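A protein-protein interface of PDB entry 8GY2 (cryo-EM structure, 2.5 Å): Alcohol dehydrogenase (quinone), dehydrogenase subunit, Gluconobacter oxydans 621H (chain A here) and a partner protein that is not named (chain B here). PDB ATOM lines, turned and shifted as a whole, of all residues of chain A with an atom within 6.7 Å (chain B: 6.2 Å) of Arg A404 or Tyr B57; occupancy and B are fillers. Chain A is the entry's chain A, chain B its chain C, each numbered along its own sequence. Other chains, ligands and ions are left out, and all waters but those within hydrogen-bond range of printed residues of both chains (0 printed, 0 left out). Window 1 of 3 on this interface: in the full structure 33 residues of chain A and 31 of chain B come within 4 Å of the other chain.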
ATOM      1  N   ASP A 312     -10.372  -8.325 -11.999  1.00  0.00           N
ATOM      2  CA  ASP A 312     -11.288  -9.220 -11.306  1.00  0.00           C
ATOM      3  C   ASP A 312     -10.736 -10.628 -11.143  1.00  0.00           C
ATOM      4  O   ASP A 312     -11.264 -11.388 -10.324  1.00  0.00           O
ATOM      5  CB  ASP A 312     -12.623  -9.290 -12.049  1.00  0.00           C
ATOM      6  CG  ASP A 312     -13.734  -8.570 -11.318  1.00  0.00           C
ATOM      7  OD1 ASP A 312     -13.527  -8.189 -10.147  1.00  0.00           O
ATOM      8  OD2 ASP A 312     -14.817  -8.389 -11.911  1.00  0.00           O
ATOM      9  N   PHE A 333     -20.434 -17.314 -12.842  1.00  0.00           N
ATOM     10  CA  PHE A 333     -20.824 -16.337 -11.830  1.00  0.00           C
ATOM     11  C   PHE A 333     -19.717 -16.257 -10.794  1.00  0.00           C
ATOM     12  O   PHE A 333     -19.400 -17.260 -10.147  1.00  0.00           O
ATOM     13  CB  PHE A 333     -22.153 -16.708 -11.165  1.00  0.00           C
ATOM     14  CG  PHE A 333     -22.532 -15.800 -10.031  1.00  0.00           C
ATOM     15  CD1 PHE A 333     -22.962 -14.506 -10.277  1.00  0.00           C
ATOM     16  CD2 PHE A 333     -22.451 -16.234  -8.720  1.00  0.00           C
ATOM     17  CE1 PHE A 333     -23.307 -13.666  -9.237  1.00  0.00           C
ATOM     18  CE2 PHE A 333     -22.795 -15.398  -7.676  1.00  0.00           C
ATOM     19  CZ  PHE A 333     -23.223 -14.113  -7.936  1.00  0.00           C
ATOM     20  N   GLN A 334     -19.130 -15.071 -10.636  1.00  0.00           N
ATOM     21  CA  GLN A 334     -18.022 -14.869  -9.709  1.00  0.00           C
ATOM     22  C   GLN A 334     -18.575 -14.444  -8.355  1.00  0.00           C
ATOM     23  O   GLN A 334     -19.079 -13.326  -8.203  1.00  0.00           O
ATOM     24  CB  GLN A 334     -17.039 -13.835 -10.250  1.00  0.00           C
ATOM     25  CG  GLN A 334     -15.643 -13.968  -9.667  1.00  0.00           C
ATOM     26  CD  GLN A 334     -14.698 -12.895 -10.158  1.00  0.00           C
ATOM     27  OE1 GLN A 334     -15.124 -11.821 -10.576  1.00  0.00           O
ATOM     28  NE2 GLN A 334     -13.403 -13.182 -10.110  1.00  0.00           N
ATOM     29  N   GLU A 335     -18.482 -15.340  -7.373  1.00  0.00           N
ATOM     30  CA  GLU A 335     -18.975 -15.036  -6.036  1.00  0.00           C
ATOM     31  C   GLU A 335     -18.016 -14.130  -5.271  1.00  0.00           C
ATOM     32  O   GLU A 335     -18.455 -13.261  -4.511  1.00  0.00           O
ATOM     33  CB  GLU A 335     -19.218 -16.331  -5.265  1.00  0.00           C
ATOM     34  CG  GLU A 335     -20.169 -17.287  -5.964  1.00  0.00           C
ATOM     35  CD  GLU A 335     -20.215 -18.649  -5.305  1.00  0.00           C
ATOM     36  OE1 GLU A 335     -19.277 -18.975  -4.551  1.00  0.00           O
ATOM     37  OE2 GLU A 335     -21.189 -19.392  -5.542  1.00  0.00           O
ATOM     38  N   PRO A 337     -14.981 -11.822  -6.269  1.00  0.00           N
ATOM     39  CA  PRO A 337     -13.978 -11.121  -7.079  1.00  0.00           C
ATOM     40  C   PRO A 337     -12.802 -10.664  -6.230  1.00  0.00           C
ATOM     41  O   PRO A 337     -12.949 -10.344  -5.048  1.00  0.00           O
ATOM     42  CB  PRO A 337     -14.751  -9.925  -7.648  1.00  0.00           C
ATOM     43  CG  PRO A 337     -16.184 -10.319  -7.569  1.00  0.00           C
ATOM     44  CD  PRO A 337     -16.309 -11.191  -6.360  1.00  0.00           C
ATOM     45  N   MET A 338     -11.626 -10.611  -6.862  1.00  0.00           N
ATOM     46  CA  MET A 338     -10.377 -10.190  -6.219  1.00  0.00           C
ATOM     47  C   MET A 338     -10.178 -10.888  -4.876  1.00  0.00           C
ATOM     48  O   MET A 338      -9.913 -10.257  -3.851  1.00  0.00           O
ATOM     49  CB  MET A 338     -10.319  -8.668  -6.052  1.00  0.00           C
ATOM     50  CG  MET A 338     -11.319  -7.879  -6.878  1.00  0.00           C
ATOM     51  SD  MET A 338     -11.279  -6.124  -6.486  1.00  0.00           S
ATOM     52  CE  MET A 338     -12.133  -6.131  -4.913  1.00  0.00           C
ATOM     53  N   PHE A 383     -27.836 -14.390 -11.412  1.00  0.00           N
ATOM     54  CA  PHE A 383     -27.879 -14.251  -9.964  1.00  0.00           C
ATOM     55  C   PHE A 383     -29.307 -13.972  -9.510  1.00  0.00           C
ATOM     56  O   PHE A 383     -29.978 -13.086 -10.048  1.00  0.00           O
ATOM     57  CB  PHE A 383     -26.942 -13.126  -9.523  1.00  0.00           C
ATOM     58  CG  PHE A 383     -27.117 -12.706  -8.091  1.00  0.00           C
ATOM     59  CD1 PHE A 383     -26.534 -13.430  -7.067  1.00  0.00           C
ATOM     60  CD2 PHE A 383     -27.842 -11.571  -7.773  1.00  0.00           C
ATOM     61  CE1 PHE A 383     -26.686 -13.040  -5.751  1.00  0.00           C
ATOM     62  CE2 PHE A 383     -27.997 -11.177  -6.459  1.00  0.00           C
ATOM     63  CZ  PHE A 383     -27.417 -11.912  -5.448  1.00  0.00           C
ATOM     64  N   GLY A 397     -23.134  -7.194   2.836  1.00  0.00           N
ATOM     65  CA  GLY A 397     -24.059  -7.831   1.929  1.00  0.00           C
ATOM     66  C   GLY A 397     -23.547  -7.815   0.501  1.00  0.00           C
ATOM     67  O   GLY A 397     -22.379  -7.535   0.219  1.00  0.00           O
ATOM     68  N   LEU A 398     -24.453  -8.127  -0.418  1.00  0.00           N
ATOM     69  CA  LEU A 398     -24.151  -8.154  -1.838  1.00  0.00           C
ATOM     70  C   LEU A 398     -24.911  -7.050  -2.560  1.00  0.00           C
ATOM     71  O   LEU A 398     -25.885  -6.495  -2.046  1.00  0.00           O
ATOM     72  CB  LEU A 398     -24.503  -9.512  -2.452  1.00  0.00           C
ATOM     73  CG  LEU A 398     -23.968 -10.753  -1.739  1.00  0.00           C
ATOM     74  CD1 LEU A 398     -24.601 -11.999  -2.323  1.00  0.00           C
ATOM     75  CD2 LEU A 398     -22.456 -10.821  -1.843  1.00  0.00           C
ATOM     76  N   ASP A 399     -24.450  -6.738  -3.760  1.00  0.00           N
ATOM     77  CA  ASP A 399     -25.131  -5.760  -4.596  1.00  0.00           C
ATOM     78  C   ASP A 399     -26.417  -6.370  -5.135  1.00  0.00           C
ATOM     79  O   ASP A 399     -26.361  -7.404  -5.813  1.00  0.00           O
ATOM     80  CB  ASP A 399     -24.221  -5.321  -5.738  1.00  0.00           C
ATOM     81  CG  ASP A 399     -24.684  -4.041  -6.398  1.00  0.00           C
ATOM     82  OD1 ASP A 399     -25.604  -3.389  -5.864  1.00  0.00           O
ATOM     83  OD2 ASP A 399     -24.123  -3.683  -7.454  1.00  0.00           O
ATOM     84  N   PRO A 400     -27.585  -5.785  -4.860  1.00  0.00           N
ATOM     85  CA  PRO A 400     -28.836  -6.380  -5.359  1.00  0.00           C
ATOM     86  C   PRO A 400     -28.943  -6.410  -6.872  1.00  0.00           C
ATOM     87  O   PRO A 400     -29.756  -7.178  -7.402  1.00  0.00           O
ATOM     88  CB  PRO A 400     -29.922  -5.490  -4.738  1.00  0.00           C
ATOM     89  CG  PRO A 400     -29.222  -4.228  -4.352  1.00  0.00           C
ATOM     90  CD  PRO A 400     -27.832  -4.630  -3.985  1.00  0.00           C
ATOM     91  N   VAL A 401     -28.159  -5.604  -7.587  1.00  0.00           N
ATOM     92  CA  VAL A 401     -28.272  -5.532  -9.039  1.00  0.00           C
ATOM     93  C   VAL A 401     -27.251  -6.403  -9.769  1.00  0.00           C
ATOM     94  O   VAL A 401     -27.452  -6.703 -10.955  1.00  0.00           O
ATOM     95  CB  VAL A 401     -28.162  -4.071  -9.524  1.00  0.00           C
ATOM     96  CG1 VAL A 401     -29.077  -3.173  -8.707  1.00  0.00           C
ATOM     97  CG2 VAL A 401     -26.728  -3.588  -9.442  1.00  0.00           C
ATOM     98  N   THR A 402     -26.170  -6.816  -9.105  1.00  0.00           N
ATOM     99  CA  THR A 402     -25.148  -7.623  -9.762  1.00  0.00           C
ATOM    100  C   THR A 402     -24.828  -8.883  -8.971  1.00  0.00           C
ATOM    101  O   THR A 402     -24.447  -9.905  -9.549  1.00  0.00           O
ATOM    102  CB  THR A 402     -23.863  -6.815  -9.963  1.00  0.00           C
ATOM    103  OG1 THR A 402     -23.442  -6.263  -8.710  1.00  0.00           O
ATOM    104  CG2 THR A 402     -24.081  -5.694 -10.955  1.00  0.00           C
ATOM    105  N   GLY A 403     -24.975  -8.821  -7.652  1.00  0.00           N
ATOM    106  CA  GLY A 403     -24.504  -9.876  -6.785  1.00  0.00           C
ATOM    107  C   GLY A 403     -23.061  -9.738  -6.356  1.00  0.00           C
ATOM    108  O   GLY A 403     -22.575 -10.584  -5.596  1.00  0.00           O
ATOM    109  N   ARG A 404     -22.363  -8.709  -6.824  1.00  0.00           N
ATOM    110  CA  ARG A 404     -20.995  -8.475  -6.390  1.00  0.00           C
ATOM    111  C   ARG A 404     -20.987  -8.011  -4.935  1.00  0.00           C
ATOM    112  O   ARG A 404     -21.818  -7.186  -4.541  1.00  0.00           O
ATOM    113  CB  ARG A 404     -20.324  -7.432  -7.284  1.00  0.00           C
ATOM    114  CG  ARG A 404     -19.019  -6.875  -6.741  1.00  0.00           C
ATOM    115  CD  ARG A 404     -18.697  -5.526  -7.353  1.00  0.00           C
ATOM    116  NE  ARG A 404     -17.306  -5.146  -7.139  1.00  0.00           N
ATOM    117  CZ  ARG A 404     -16.300  -5.502  -7.926  1.00  0.00           C
ATOM    118  NH1 ARG A 404     -16.495  -6.256  -8.996  1.00  0.00           N
ATOM    119  NH2 ARG A 404     -15.070  -5.093  -7.633  1.00  0.00           N
ATOM    120  N   PRO A 405     -20.077  -8.531  -4.111  1.00  0.00           N
ATOM    121  CA  PRO A 405     -20.057  -8.141  -2.697  1.00  0.00           C
ATOM    122  C   PRO A 405     -19.759  -6.661  -2.518  1.00  0.00           C
ATOM    123  O   PRO A 405     -19.017  -6.053  -3.293  1.00  0.00           O
ATOM    124  CB  PRO A 405     -18.939  -9.008  -2.105  1.00  0.00           C
ATOM    125  CG  PRO A 405     -18.753 -10.125  -3.075  1.00  0.00           C
ATOM    126  CD  PRO A 405     -19.072  -9.561  -4.419  1.00  0.00           C
ATOM    127  N   ASN A 406     -20.357  -6.080  -1.479  1.00  0.00           N
ATOM    128  CA  ASN A 406     -20.074  -4.701  -1.087  1.00  0.00           C
ATOM    129  C   ASN A 406     -18.933  -4.742  -0.080  1.00  0.00           C
ATOM    130  O   ASN A 406     -19.147  -4.765   1.132  1.00  0.00           O
ATOM    131  CB  ASN A 406     -21.312  -4.028  -0.509  1.00  0.00           C
ATOM    132  CG  ASN A 406     -22.555  -4.298  -1.326  1.00  0.00           C
ATOM    133  OD1 ASN A 406     -22.574  -4.082  -2.536  1.00  0.00           O
ATOM    134  ND2 ASN A 406     -23.606  -4.765  -0.666  1.00  0.00           N
ATOM    135  N   TYR A 407     -17.705  -4.757  -0.593  1.00  0.00           N
ATOM    136  CA  TYR A 407     -16.534  -4.869   0.264  1.00  0.00           C
ATOM    137  C   TYR A 407     -16.452  -3.693   1.227  1.00  0.00           C
ATOM    138  O   TYR A 407     -16.728  -2.548   0.860  1.00  0.00           O
ATOM    139  CB  TYR A 407     -15.258  -4.917  -0.574  1.00  0.00           C
ATOM    140  CG  TYR A 407     -15.205  -6.016  -1.606  1.00  0.00           C
ATOM    141  CD1 TYR A 407     -15.692  -5.814  -2.889  1.00  0.00           C
ATOM    142  CD2 TYR A 407     -14.648  -7.249  -1.304  1.00  0.00           C
ATOM    143  CE1 TYR A 407     -15.637  -6.813  -3.838  1.00  0.00           C
ATOM    144  CE2 TYR A 407     -14.590  -8.253  -2.245  1.00  0.00           C
ATOM    145  CZ  TYR A 407     -15.084  -8.030  -3.508  1.00  0.00           C
ATOM    146  OH  TYR A 407     -15.025  -9.030  -4.447  1.00  0.00           O
ATOM    147  N   ALA B  52      -7.712   6.179  -8.780  1.00  0.00           N
ATOM    148  CA  ALA B  52      -7.133   4.928  -9.257  1.00  0.00           C
ATOM    149  C   ALA B  52      -7.929   3.731  -8.758  1.00  0.00           C
ATOM    150  O   ALA B  52      -8.180   2.784  -9.513  1.00  0.00           O
ATOM    151  CB  ALA B  52      -5.673   4.824  -8.820  1.00  0.00           C
ATOM    152  N   GLY B  53      -8.345   3.755  -7.492  1.00  0.00           N
ATOM    153  CA  GLY B  53      -9.203   2.694  -6.991  1.00  0.00           C
ATOM    154  C   GLY B  53     -10.555   2.669  -7.677  1.00  0.00           C
ATOM    155  O   GLY B  53     -11.085   1.599  -7.991  1.00  0.00           O
ATOM    156  N   ILE B  54     -11.133   3.849  -7.917  1.00  0.00           N
ATOM    157  CA  ILE B  54     -12.420   3.924  -8.602  1.00  0.00           C
ATOM    158  C   ILE B  54     -12.310   3.343 -10.005  1.00  0.00           C
ATOM    159  O   ILE B  54     -13.196   2.614 -10.462  1.00  0.00           O
ATOM    160  CB  ILE B  54     -12.931   5.378  -8.619  1.00  0.00           C
ATOM    161  CG1 ILE B  54     -13.491   5.766  -7.249  1.00  0.00           C
ATOM    162  CG2 ILE B  54     -13.990   5.568  -9.691  1.00  0.00           C
ATOM    163  CD1 ILE B  54     -14.790   5.068  -6.902  1.00  0.00           C
ATOM    164  N   MET B  55     -11.215   3.638 -10.707  1.00  0.00           N
ATOM    165  CA  MET B  55     -11.003   3.067 -12.029  1.00  0.00           C
ATOM    166  C   MET B  55     -10.644   1.589 -11.987  1.00  0.00           C
ATOM    167  O   MET B  55     -10.871   0.889 -12.974  1.00  0.00           O
ATOM    168  CB  MET B  55      -9.919   3.844 -12.781  1.00  0.00           C
ATOM    169  CG  MET B  55     -10.152   3.967 -14.290  1.00  0.00           C
ATOM    170  SD  MET B  55     -11.829   4.252 -14.919  1.00  0.00           S
ATOM    171  CE  MET B  55     -12.523   5.459 -13.787  1.00  0.00           C
ATOM    172  N   ASN B  56     -10.073   1.099 -10.888  1.00  0.00           N
ATOM    173  CA  ASN B  56      -9.960  -0.346 -10.720  1.00  0.00           C
ATOM    174  C   ASN B  56     -11.339  -0.981 -10.596  1.00  0.00           C
ATOM    175  O   ASN B  56     -11.594  -2.051 -11.159  1.00  0.00           O
ATOM    176  CB  ASN B  56      -9.107  -0.679  -9.498  1.00  0.00           C
ATOM    177  CG  ASN B  56      -8.993  -2.172  -9.259  1.00  0.00           C
ATOM    178  OD1 ASN B  56      -8.894  -2.955 -10.201  1.00  0.00           O
ATOM    179  ND2 ASN B  56      -9.011  -2.572  -7.994  1.00  0.00           N
ATOM    180  N   TYR B  57     -12.236  -0.328  -9.855  1.00  0.00           N
ATOM    181  CA  TYR B  57     -13.607  -0.811  -9.730  1.00  0.00           C
ATOM    182  C   TYR B  57     -14.361  -0.726 -11.051  1.00  0.00           C
ATOM    183  O   TYR B  57     -15.236  -1.555 -11.320  1.00  0.00           O
ATOM    184  CB  TYR B  57     -14.333  -0.015  -8.643  1.00  0.00           C
ATOM    185  CG  TYR B  57     -15.838  -0.172  -8.630  1.00  0.00           C
ATOM    186  CD1 TYR B  57     -16.440  -1.229  -7.962  1.00  0.00           C
ATOM    187  CD2 TYR B  57     -16.659   0.751  -9.266  1.00  0.00           C
ATOM    188  CE1 TYR B  57     -17.814  -1.372  -7.942  1.00  0.00           C
ATOM    189  CE2 TYR B  57     -18.033   0.615  -9.251  1.00  0.00           C
ATOM    190  CZ  TYR B  57     -18.604  -0.447  -8.587  1.00  0.00           C
ATOM    191  OH  TYR B  57     -19.971  -0.586  -8.569  1.00  0.00           O
ATOM    192  N   CYS B  58     -14.044   0.270 -11.878  1.00  0.00           N
ATOM    193  CA  CYS B  58     -14.755   0.489 -13.133  1.00  0.00           C
ATOM    194  C   CYS B  58     -14.166  -0.285 -14.307  1.00  0.00           C
ATOM    195  O   CYS B  58     -14.881  -0.554 -15.274  1.00  0.00           O
ATOM    196  CB  CYS B  58     -14.779   1.983 -13.473  1.00  0.00           C
ATOM    197  SG  CYS B  58     -15.805   2.993 -12.376  1.00  0.00           S
ATOM    198  N   VAL B  59     -12.880  -0.631 -14.275  1.00  0.00           N
ATOM    199  CA  VAL B  59     -12.321  -1.454 -15.344  1.00  0.00           C
ATOM    200  C   VAL B  59     -12.897  -2.861 -15.269  1.00  0.00           C
ATOM    201  O   VAL B  59     -13.335  -3.427 -16.276  1.00  0.00           O
ATOM    202  CB  VAL B  59     -10.784  -1.457 -15.278  1.00  0.00           C
ATOM    203  CG1 VAL B  59     -10.223  -2.726 -15.896  1.00  0.00           C
ATOM    204  CG2 VAL B  59     -10.229  -0.231 -15.982  1.00  0.00           C
ATOM    205  N   GLU B  60     -12.914  -3.440 -14.072  1.00  0.00           N
ATOM    206  CA  GLU B  60     -13.738  -4.611 -13.834  1.00  0.00           C
ATOM    207  C   GLU B  60     -15.201  -4.189 -13.765  1.00  0.00           C
ATOM    208  O   GLU B  60     -15.522  -3.006 -13.623  1.00  0.00           O
ATOM    209  CB  GLU B  60     -13.315  -5.315 -12.545  1.00  0.00           C
ATOM    210  CG  GLU B  60     -13.596  -4.526 -11.281  1.00  0.00           C
ATOM    211  CD  GLU B  60     -12.668  -4.899 -10.142  1.00  0.00           C
ATOM    212  OE1 GLU B  60     -11.610  -5.504 -10.407  1.00  0.00           O
ATOM    213  OE2 GLU B  60     -12.997  -4.585  -8.979  1.00  0.00           O
ATOM    214  N   GLN B  61     -16.094  -5.169 -13.918  1.00  0.00           N
ATOM    215  CA  GLN B  61     -17.535  -4.927 -13.923  1.00  0.00           C
ATOM    216  C   GLN B  61     -17.939  -4.059 -15.114  1.00  0.00           C
ATOM    217  O   GLN B  61     -19.115  -3.718 -15.273  1.00  0.00           O
ATOM    218  CB  GLN B  61     -17.975  -4.277 -12.602  1.00  0.00           C
ATOM    219  CG  GLN B  61     -19.474  -4.235 -12.366  1.00  0.00           C
ATOM    220  CD  GLN B  61     -19.833  -4.440 -10.913  1.00  0.00           C
ATOM    221  OE1 GLN B  61     -19.253  -3.814 -10.026  1.00  0.00           O
ATOM    222  NE2 GLN B  61     -20.793  -5.320 -10.656  1.00  0.00           N
ATOM    223  N   GLN B  62     -16.975  -3.722 -15.963  1.00  0.00           N
ATOM    224  CA  GLN B  62     -17.159  -2.833 -17.123  1.00  0.00           C
ATOM    225  C   GLN B  62     -17.704  -1.497 -16.607  1.00  0.00           C
ATOM    226  O   GLN B  62     -17.340  -1.074 -15.501  1.00  0.00           O
ATOM    227  CB  GLN B  62     -18.015  -3.517 -18.170  1.00  0.00           C
ATOM    228  CG  GLN B  62     -17.389  -4.757 -18.801  1.00  0.00           C
ATOM    229  CD  GLN B  62     -15.880  -4.803 -18.658  1.00  0.00           C
ATOM    230  OE1 GLN B  62     -15.156  -4.073 -19.338  1.00  0.00           O
ATOM    231  NE2 GLN B  62     -15.397  -5.669 -17.777  1.00  0.00           N
ATOM    232  N   TYR B  63     -18.611  -0.860 -17.344  1.00  0.00           N
ATOM    233  CA  TYR B  63     -19.132   0.500 -17.229  1.00  0.00           C
ATOM    234  C   TYR B  63     -18.199   1.553 -17.826  1.00  0.00           C
ATOM    235  O   TYR B  63     -18.619   2.705 -17.949  1.00  0.00           O
ATOM    236  CB  TYR B  63     -19.444   0.929 -15.780  1.00  0.00           C
ATOM    237  CG  TYR B  63     -20.272  -0.031 -14.961  1.00  0.00           C
ATOM    238  CD1 TYR B  63     -21.274  -0.795 -15.540  1.00  0.00           C
ATOM    239  CD2 TYR B  63     -20.055  -0.161 -13.596  1.00  0.00           C
ATOM    240  CE1 TYR B  63     -22.032  -1.666 -14.781  1.00  0.00           C
ATOM    241  CE2 TYR B  63     -20.805  -1.026 -12.833  1.00  0.00           C
ATOM    242  CZ  TYR B  63     -21.791  -1.777 -13.429  1.00  0.00           C
ATOM    243  OH  TYR B  63     -22.540  -2.641 -12.666  1.00  0.00           O
ATOM    244  N   GLY B  95     -12.332   2.919  -2.830  1.00  0.00           N
ATOM    245  CA  GLY B  95     -12.397   3.239  -4.240  1.00  0.00           C
ATOM    246  C   GLY B  95     -12.365   1.983  -5.079  1.00  0.00           C
ATOM    247  O   GLY B  95     -12.986   1.929  -6.143  1.00  0.00           O
ATOM    248  N   THR B  96     -11.662   0.954  -4.603  1.00  0.00           N
ATOM    249  CA  THR B  96     -11.869  -0.376  -5.161  1.00  0.00           C
ATOM    250  C   THR B  96     -13.296  -0.839  -4.900  1.00  0.00           C
ATOM    251  O   THR B  96     -13.892  -1.528  -5.736  1.00  0.00           O
ATOM    252  CB  THR B  96     -10.855  -1.358  -4.577  1.00  0.00           C
ATOM    253  OG1 THR B  96      -9.530  -0.908  -4.882  1.00  0.00           O
ATOM    254  CG2 THR B  96     -11.045  -2.738  -5.171  1.00  0.00           C
ATOM    255  N   ALA B  97     -13.856  -0.459  -3.756  1.00  0.00           N
ATOM    256  CA  ALA B  97     -15.292  -0.528  -3.526  1.00  0.00           C
ATOM    257  C   ALA B  97     -15.942   0.694  -4.178  1.00  0.00           C
ATOM    258  O   ALA B  97     -15.326   1.398  -4.980  1.00  0.00           O
ATOM    259  CB  ALA B  97     -15.586  -0.619  -2.032  1.00  0.00           C
ATOM    260  N   GLY B  98     -17.196   0.963  -3.852  1.00  0.00           N
ATOM    261  CA  GLY B  98     -17.845   2.099  -4.475  1.00  0.00           C
ATOM    262  C   GLY B  98     -17.578   3.449  -3.847  1.00  0.00           C
ATOM    263  O   GLY B  98     -18.118   4.451  -4.322  1.00  0.00           O
ATOM    264  N   LEU B 109     -20.616   4.406  -4.987  1.00  0.00           N
ATOM    265  CA  LEU B 109     -20.949   4.033  -6.355  1.00  0.00           C
ATOM    266  C   LEU B 109     -21.787   2.765  -6.446  1.00  0.00           C
ATOM    267  O   LEU B 109     -22.380   2.509  -7.498  1.00  0.00           O
ATOM    268  CB  LEU B 109     -19.676   3.855  -7.186  1.00  0.00           C
ATOM    269  CG  LEU B 109     -19.147   5.091  -7.917  1.00  0.00           C
ATOM    270  CD1 LEU B 109     -18.219   4.680  -9.047  1.00  0.00           C
ATOM    271  CD2 LEU B 109     -20.288   5.946  -8.444  1.00  0.00           C
ATOM    272  N   VAL B 110     -21.844   1.961  -5.378  1.00  0.00           N
ATOM    273  CA  VAL B 110     -22.732   0.798  -5.359  1.00  0.00           C
ATOM    274  C   VAL B 110     -24.183   1.210  -5.172  1.00  0.00           C
ATOM    275  O   VAL B 110     -25.086   0.375  -5.306  1.00  0.00           O
ATOM    276  CB  VAL B 110     -22.248  -0.195  -4.285  1.00  0.00           C
ATOM    277  CG1 VAL B 110     -22.982  -1.519  -4.390  1.00  0.00           C
ATOM    278  CG2 VAL B 110     -20.757  -0.429  -4.443  1.00  0.00           C
ATOM    279  N   ARG B 118     -24.127   4.332 -12.978  1.00  0.00           N
ATOM    280  CA  ARG B 118     -22.785   3.823 -12.717  1.00  0.00           C
ATOM    281  C   ARG B 118     -21.868   4.133 -13.892  1.00  0.00           C
ATOM    282  O   ARG B 118     -20.727   4.573 -13.710  1.00  0.00           O
ATOM    283  CB  ARG B 118     -22.834   2.319 -12.444  1.00  0.00           C
ATOM    284  CG  ARG B 118     -23.067   1.961 -10.985  1.00  0.00           C
ATOM    285  CD  ARG B 118     -23.583   0.539 -10.845  1.00  0.00           C
ATOM    286  NE  ARG B 118     -24.401   0.367  -9.651  1.00  0.00           N
ATOM    287  CZ  ARG B 118     -24.490  -0.762  -8.961  1.00  0.00           C
ATOM    288  NH1 ARG B 118     -23.818  -1.845  -9.316  1.00  0.00           N
ATOM    289  NH2 ARG B 118     -25.274  -0.806  -7.887  1.00  0.00           N
ATOM    290  N   CYS B 122     -18.180   6.482 -14.038  1.00  0.00           N
ATOM    291  CA  CYS B 122     -16.831   6.052 -14.386  1.00  0.00           C
ATOM    292  C   CYS B 122     -16.264   6.904 -15.515  1.00  0.00           C
ATOM    293  O   CYS B 122     -15.067   7.213 -15.527  1.00  0.00           O
ATOM    294  CB  CYS B 122     -16.828   4.572 -14.769  1.00  0.00           C
ATOM    295  SG  CYS B 122     -17.444   3.456 -13.485  1.00  0.00           S
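Of chain B, only Tyr B57 (3.9 Å), Glu B60 (2.5 Å) and Gln B61 (3.2 Å) come within 4 Å of Arg A404. Tyr B57 touches just one residue of chain A: Arg A404 (3.9 Å). Of the printed residues of chain A, Tyr B63 touches Thr A402. Of the printed residues of chain A, Ala B97 touches Tyr A407 (3.7 Å). The nearest residue of chain A that does not touch Tyr B57 is Asp A399 (5.3 Å). The nearest printed residue of chain A that does not touch Val B110 is Pro A400 (5.8 Å).
The guanidinium group of Arg A404 is in salt-bridge range of the side-chain carboxylate of Glu B60 (2.5 Å). The side-chain carboxylate (OE1) of Glu B60 lies within hydrogen-bond range of the backbone NH (N) of Asp A312. OG1 of Thr A402 lies close to NE2 of Gln B61 (3.4 Å). SD of Met A338 lies close to OE2 of Glu B60, 3.4 Å away. The guanidinium group (NH1) of Arg B118 is in salt-bridge range of the side-chain carboxylate (OD2) of Asp A399 (2.6 Å).
The side-chain amide nitrogen of Gln A334 lies within hydrogen-bond range of the backbone carbonyl oxygen of Asp A312 (2.8 Å). The guanidinium group (NH1) of Arg A404 lies within salt-bridge range of the side-chain carboxylate (OD1) of Asp A312. N of Asn A406 lies within hydrogen-bond range of O of Gly A397, 3.0 Å away. The side-chain sulfur of Cys B122 is disulfide-bonded to the side-chain sulfur of Cys B58, at 2.0 Å. O of Arg A404 lies within hydrogen-bond range of N of Asp A399. The backbone carbonyl oxygen (O) of Pro A337 sits at hydrogen-bond distance from the side-chain hydroxyl (OH) of Tyr A407, 2.5 Å away.
Among the printed residues, pairs that only touch across the chains: Asn A406 with Val B110, Arg A404 with Gln B61, Val A401 with Arg B118, Asp A399 with Val B110, Met A338 with Thr B96, Tyr A407 with Ala B97, Thr A402 with Tyr B63 and Arg A404 with Tyr B57.
Printed residues of chain A that touch a printed residue of chain B: Asp A312, Met A338, Asp A399, Val A401, Thr A402, Arg A404, Asn A406 and Tyr A407. Hydrophobic or aromatic side chains of chain A within 4 Å of the printed part of chain B: Met A338 and Val A401. Among the printed residues, 13 pairs touch across the chains. Among the printed residues, Asp or Glu carboxylates within 4 Å of a Lys or Arg side-chain nitrogen of the other chain: Asp A399 with Arg B118 and Arg A404 with Glu B60.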
